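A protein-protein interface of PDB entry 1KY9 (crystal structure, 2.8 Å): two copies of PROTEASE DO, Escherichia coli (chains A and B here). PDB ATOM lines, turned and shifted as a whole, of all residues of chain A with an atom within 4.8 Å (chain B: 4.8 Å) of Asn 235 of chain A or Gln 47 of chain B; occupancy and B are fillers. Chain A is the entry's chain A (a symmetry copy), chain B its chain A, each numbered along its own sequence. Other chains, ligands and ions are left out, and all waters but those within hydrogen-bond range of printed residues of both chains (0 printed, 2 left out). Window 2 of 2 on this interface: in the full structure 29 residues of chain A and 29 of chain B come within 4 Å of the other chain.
O of Arg 207 of chain A lies within hydrogen-bond range of ND2 of Asn 45 of chain B. O of Gly 208 of chain A sits at hydrogen-bond distance from ND2 of Asn 45 of chain B (3.1 Å). The side-chain amide nitrogen (ND2) of Asn 45 of chain B lies close to the backbone carbonyl oxygen (O) of Gly 233 of chain A (3.2 Å). The guanidinium group (NE) of Arg 207 of chain A lies within hydrogen-bond range of the backbone carbonyl oxygen (O) of Gln 47 of chain B, at 3.1 Å. The side-chain amide nitrogen (NE2) of Gln 47 of chain B sits at hydrogen-bond distance from the backbone carbonyl oxygen (O) of Asn 235 of chain A (2.6 Å). The side-chain amide nitrogen (NE2) of Gln 48 of chain B lies within hydrogen-bond range of the backbone carbonyl oxygen (O) of Arg 207 of chain A (2.5 Å).
The backbone NH of Gln 47 of chain B sits close to the side-chain amide oxygen of Asn 45 of chain B (3.0 Å). The backbone carbonyl oxygen (O) of Ile 205 of chain A sits at hydrogen-bond distance from the side-chain amide nitrogen (ND2) of Asn 235 of chain A, at 2.5 Å. The guanidinium group (NH1) of Arg 207 of chain A lies close to the side-chain amide oxygen (OD1) of Asn 206 of chain A, 3.5 Å away. The side-chain amide nitrogen of Asn 235 of chain A is in hydrogen-bond range of the backbone carbonyl oxygen of Gly 208 of chain A (3.4 Å).
Among the printed residues, pairs that only touch across the chains: Gly 208 of chain A with Gln 48 of chain B (3.6 Å), Arg 207 of chain A with Phe 49 of chain B (3.8 Å) and Gly 234 of chain A with Asn 45 of chain B (3.8 Å).
Asn 235 of chain A touches just one residue of chain B: Gln 47 (2.6 Å). Gln 47 of chain B touches just these residues of chain A: Arg 207 and Asn 235. Of the printed residues of chain B, Gly 233 of chain A touches Asn 45 (3.0 Å). Of the printed residues of chain B, Gly 208 of chain A touches Asn 45 and Gln 48. Printed residues of chain A within 4 Å of Gln 48 of chain B: Arg 207 (2.5 Å) and Gly 208 (3.6 Å). Ile 236 of chain A touches none of the printed residues of chain B. The nearest residue of chain A that does not touch Gln 47 of chain B is Gly 234 of chain A (4.4 Å).
Hydrophobic or aromatic side chains of chain B within 4 Å of the printed part of chain A: Phe 49.
No position is printed for both chains.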
ATOM      1  N   ALA A 204      -5.796 -15.041  -5.538  1.00  0.00           N
ATOM      2  CA  ALA A 204      -6.800 -14.615  -6.496  1.00  0.00           C
ATOM      3  C   ALA A 204      -8.141 -14.746  -5.815  1.00  0.00           C
ATOM      4  O   ALA A 204      -8.428 -15.783  -5.215  1.00  0.00           O
ATOM      5  CB  ALA A 204      -6.742 -15.498  -7.736  1.00  0.00           C
ATOM      6  N   ILE A 205      -8.965 -13.704  -5.900  1.00  0.00           N
ATOM      7  CA  ILE A 205     -10.281 -13.718  -5.246  1.00  0.00           C
ATOM      8  C   ILE A 205     -11.431 -14.479  -5.927  1.00  0.00           C
ATOM      9  O   ILE A 205     -11.707 -14.331  -7.120  1.00  0.00           O
ATOM     10  CB  ILE A 205     -10.760 -12.273  -4.907  1.00  0.00           C
ATOM     11  CG1 ILE A 205      -9.795 -11.209  -5.489  1.00  0.00           C
ATOM     12  CG2 ILE A 205     -10.814 -12.110  -3.396  1.00  0.00           C
ATOM     13  CD1 ILE A 205      -9.653 -11.168  -7.037  1.00  0.00           C
ATOM     14  N   ASN A 206     -12.095 -15.300  -5.120  1.00  0.00           N
ATOM     15  CA  ASN A 206     -13.230 -16.124  -5.544  1.00  0.00           C
ATOM     16  C   ASN A 206     -14.381 -15.288  -6.129  1.00  0.00           C
ATOM     17  O   ASN A 206     -14.815 -14.292  -5.541  1.00  0.00           O
ATOM     18  CB  ASN A 206     -13.723 -16.955  -4.332  1.00  0.00           C
ATOM     19  CG  ASN A 206     -14.969 -17.810  -4.635  1.00  0.00           C
ATOM     20  OD1 ASN A 206     -16.101 -17.317  -4.669  1.00  0.00           O
ATOM     21  ND2 ASN A 206     -14.756 -19.100  -4.848  1.00  0.00           N
ATOM     22  N   ARG A 207     -14.868 -15.691  -7.295  1.00  0.00           N
ATOM     23  CA  ARG A 207     -15.975 -14.988  -7.921  1.00  0.00           C
ATOM     24  C   ARG A 207     -15.680 -13.542  -8.313  1.00  0.00           C
ATOM     25  O   ARG A 207     -16.597 -12.794  -8.655  1.00  0.00           O
ATOM     26  CB  ARG A 207     -17.183 -15.003  -6.990  1.00  0.00           C
ATOM     27  CG  ARG A 207     -17.795 -16.348  -6.801  1.00  0.00           C
ATOM     28  CD  ARG A 207     -19.014 -16.259  -5.908  1.00  0.00           C
ATOM     29  NE  ARG A 207     -20.043 -17.177  -6.379  1.00  0.00           N
ATOM     30  CZ  ARG A 207     -19.835 -18.472  -6.596  1.00  0.00           C
ATOM     31  NH1 ARG A 207     -18.633 -18.995  -6.374  1.00  0.00           N
ATOM     32  NH2 ARG A 207     -20.813 -19.236  -7.067  1.00  0.00           N
ATOM     33  N   GLY A 208     -14.420 -13.130  -8.266  1.00  0.00           N
ATOM     34  CA  GLY A 208     -14.134 -11.762  -8.648  1.00  0.00           C
ATOM     35  C   GLY A 208     -13.547 -11.637 -10.044  1.00  0.00           C
ATOM     36  O   GLY A 208     -13.250 -12.643 -10.705  1.00  0.00           O
ATOM     37  N   LEU A 229     -10.957 -16.218 -19.356  1.00  0.00           N
ATOM     38  CA  LEU A 229     -12.301 -16.348 -19.885  1.00  0.00           C
ATOM     39  C   LEU A 229     -12.736 -14.959 -20.346  1.00  0.00           C
ATOM     40  O   LEU A 229     -13.554 -14.334 -19.684  1.00  0.00           O
ATOM     41  CB  LEU A 229     -13.250 -16.807 -18.780  1.00  0.00           C
ATOM     42  CG  LEU A 229     -12.669 -17.761 -17.736  1.00  0.00           C
ATOM     43  CD1 LEU A 229     -13.732 -18.094 -16.684  1.00  0.00           C
ATOM     44  CD2 LEU A 229     -12.161 -19.014 -18.421  1.00  0.00           C
ATOM     45  N   GLY A 233     -14.648 -11.087 -17.040  1.00  0.00           N
ATOM     46  CA  GLY A 233     -13.657 -10.919 -15.997  1.00  0.00           C
ATOM     47  C   GLY A 233     -14.129 -11.961 -15.020  1.00  0.00           C
ATOM     48  O   GLY A 233     -15.201 -11.811 -14.444  1.00  0.00           O
ATOM     49  N   GLY A 234     -13.371 -13.039 -14.869  1.00  0.00           N
ATOM     50  CA  GLY A 234     -13.816 -14.099 -13.993  1.00  0.00           C
ATOM     51  C   GLY A 234     -12.732 -15.050 -13.559  1.00  0.00           C
ATOM     52  O   GLY A 234     -11.642 -15.102 -14.129  1.00  0.00           O
ATOM     53  N   ASN A 235     -13.060 -15.824 -12.538  1.00  0.00           N
ATOM     54  CA  ASN A 235     -12.135 -16.774 -11.952  1.00  0.00           C
ATOM     55  C   ASN A 235     -12.408 -18.211 -12.345  1.00  0.00           C
ATOM     56  O   ASN A 235     -13.550 -18.623 -12.533  1.00  0.00           O
ATOM     57  CB  ASN A 235     -12.178 -16.644 -10.431  1.00  0.00           C
ATOM     58  CG  ASN A 235     -10.924 -16.045  -9.873  1.00  0.00           C
ATOM     59  OD1 ASN A 235      -9.893 -16.706  -9.835  1.00  0.00           O
ATOM     60  ND2 ASN A 235     -10.991 -14.783  -9.449  1.00  0.00           N
ATOM     61  N   ILE A 236     -11.335 -18.971 -12.468  1.00  0.00           N
ATOM     62  CA  ILE A 236     -11.413 -20.374 -12.822  1.00  0.00           C
ATOM     63  C   ILE A 236     -11.178 -21.141 -11.512  1.00  0.00           C
ATOM     64  O   ILE A 236     -11.455 -22.336 -11.416  1.00  0.00           O
ATOM     65  CB  ILE A 236     -10.345 -20.702 -13.944  1.00  0.00           C
ATOM     66  CG1 ILE A 236      -9.833 -22.138 -13.815  1.00  0.00           C
ATOM     67  CG2 ILE A 236      -9.182 -19.683 -13.888  1.00  0.00           C
ATOM     68  CD1 ILE A 236      -8.949 -22.588 -14.968  1.00  0.00           C
ATOM     69  N   GLY A 237     -10.711 -20.422 -10.492  1.00  0.00           N
ATOM     70  CA  GLY A 237     -10.434 -21.036  -9.200  1.00  0.00           C
ATOM     71  C   GLY A 237      -9.046 -20.675  -8.694  1.00  0.00           C
ATOM     72  O   GLY A 237      -8.719 -20.838  -7.512  1.00  0.00           O
ATOM     73  N   ILE A 238      -8.218 -20.182  -9.608  1.00  0.00           N
ATOM     74  CA  ILE A 238      -6.851 -19.776  -9.305  1.00  0.00           C
ATOM     75  C   ILE A 238      -6.577 -18.651 -10.313  1.00  0.00           C
ATOM     76  O   ILE A 238      -7.245 -18.561 -11.363  1.00  0.00           O
ATOM     77  CB  ILE A 238      -5.856 -20.973  -9.493  1.00  0.00           C
ATOM     78  CG1 ILE A 238      -4.679 -20.845  -8.519  1.00  0.00           C
ATOM     79  CG2 ILE A 238      -5.371 -21.046 -10.956  1.00  0.00           C
ATOM     80  CD1 ILE A 238      -3.592 -21.918  -8.678  1.00  0.00           C
ATOM     81  N   GLY A 239      -5.617 -17.784 -10.000  1.00  0.00           N
ATOM     82  CA  GLY A 239      -5.329 -16.679 -10.895  1.00  0.00           C
ATOM     83  C   GLY A 239      -4.160 -16.830 -11.847  1.00  0.00           C
ATOM     84  O   GLY A 239      -3.166 -17.502 -11.531  1.00  0.00           O
ATOM     85  N   ASN B  45     -19.164 -10.792 -14.928  1.00  0.00           N
ATOM     86  CA  ASN B  45     -18.640 -11.997 -14.273  1.00  0.00           C
ATOM     87  C   ASN B  45     -19.818 -12.928 -13.965  1.00  0.00           C
ATOM     88  O   ASN B  45     -20.616 -12.656 -13.067  1.00  0.00           O
ATOM     89  CB  ASN B  45     -17.896 -11.653 -12.975  1.00  0.00           C
ATOM     90  CG  ASN B  45     -17.170 -12.855 -12.378  1.00  0.00           C
ATOM     91  OD1 ASN B  45     -17.452 -14.003 -12.722  1.00  0.00           O
ATOM     92  ND2 ASN B  45     -16.240 -12.592 -11.473  1.00  0.00           N
ATOM     93  N   PHE B  46     -19.923 -14.030 -14.701  1.00  0.00           N
ATOM     94  CA  PHE B  46     -21.040 -14.950 -14.505  1.00  0.00           C
ATOM     95  C   PHE B  46     -21.008 -15.720 -13.186  1.00  0.00           C
ATOM     96  O   PHE B  46     -21.766 -16.670 -12.999  1.00  0.00           O
ATOM     97  CB  PHE B  46     -21.145 -15.935 -15.678  1.00  0.00           C
ATOM     98  CG  PHE B  46     -20.213 -17.100 -15.578  1.00  0.00           C
ATOM     99  CD1 PHE B  46     -18.867 -16.959 -15.881  1.00  0.00           C
ATOM    100  CD2 PHE B  46     -20.679 -18.339 -15.146  1.00  0.00           C
ATOM    101  CE1 PHE B  46     -17.994 -18.038 -15.753  1.00  0.00           C
ATOM    102  CE2 PHE B  46     -19.819 -19.423 -15.012  1.00  0.00           C
ATOM    103  CZ  PHE B  46     -18.471 -19.272 -15.317  1.00  0.00           C
ATOM    104  N   GLN B  47     -20.137 -15.311 -12.273  1.00  0.00           N
ATOM    105  CA  GLN B  47     -20.045 -15.968 -10.978  1.00  0.00           C
ATOM    106  C   GLN B  47     -20.437 -14.988  -9.889  1.00  0.00           C
ATOM    107  O   GLN B  47     -20.146 -15.210  -8.712  1.00  0.00           O
ATOM    108  CB  GLN B  47     -18.624 -16.469 -10.720  1.00  0.00           C
ATOM    109  CG  GLN B  47     -18.214 -17.656 -11.571  1.00  0.00           C
ATOM    110  CD  GLN B  47     -16.740 -17.986 -11.428  1.00  0.00           C
ATOM    111  OE1 GLN B  47     -16.267 -18.320 -10.341  1.00  0.00           O
ATOM    112  NE2 GLN B  47     -16.002 -17.885 -12.529  1.00  0.00           N
ATOM    113  N   GLN B  48     -21.110 -13.911 -10.286  1.00  0.00           N
ATOM    114  CA  GLN B  48     -21.523 -12.885  -9.336  1.00  0.00           C
ATOM    115  C   GLN B  48     -22.995 -12.469  -9.379  1.00  0.00           C
ATOM    116  O   GLN B  48     -23.601 -12.365 -10.450  1.00  0.00           O
ATOM    117  CB  GLN B  48     -20.663 -11.636  -9.519  1.00  0.00           C
ATOM    118  CG  GLN B  48     -19.179 -11.889  -9.427  1.00  0.00           C
ATOM    119  CD  GLN B  48     -18.382 -10.606  -9.378  1.00  0.00           C
ATOM    120  OE1 GLN B  48     -18.553  -9.720 -10.218  1.00  0.00           O
ATOM    121  NE2 GLN B  48     -17.500 -10.498  -8.392  1.00  0.00           N
ATOM    122  N   PHE B  49     -23.546 -12.218  -8.191  1.00  0.00           N
ATOM    123  CA  PHE B  49     -24.930 -11.780  -8.018  1.00  0.00           C
ATOM    124  C   PHE B  49     -24.844 -10.260  -7.867  1.00  0.00           C
ATOM    125  O   PHE B  49     -24.610  -9.759  -6.768  1.00  0.00           O
ATOM    126  CB  PHE B  49     -25.523 -12.389  -6.740  1.00  0.00           C
ATOM    127  CG  PHE B  49     -24.815 -13.644  -6.264  1.00  0.00           C
ATOM    128  CD1 PHE B  49     -24.797 -14.802  -7.046  1.00  0.00           C
ATOM    129  CD2 PHE B  49     -24.163 -13.662  -5.026  1.00  0.00           C
ATOM    130  CE1 PHE B  49     -24.140 -15.957  -6.602  1.00  0.00           C
ATOM    131  CE2 PHE B  49     -23.504 -14.814  -4.574  1.00  0.00           C
ATOM    132  CZ  PHE B  49     -23.492 -15.962  -5.363  1.00  0.00           C
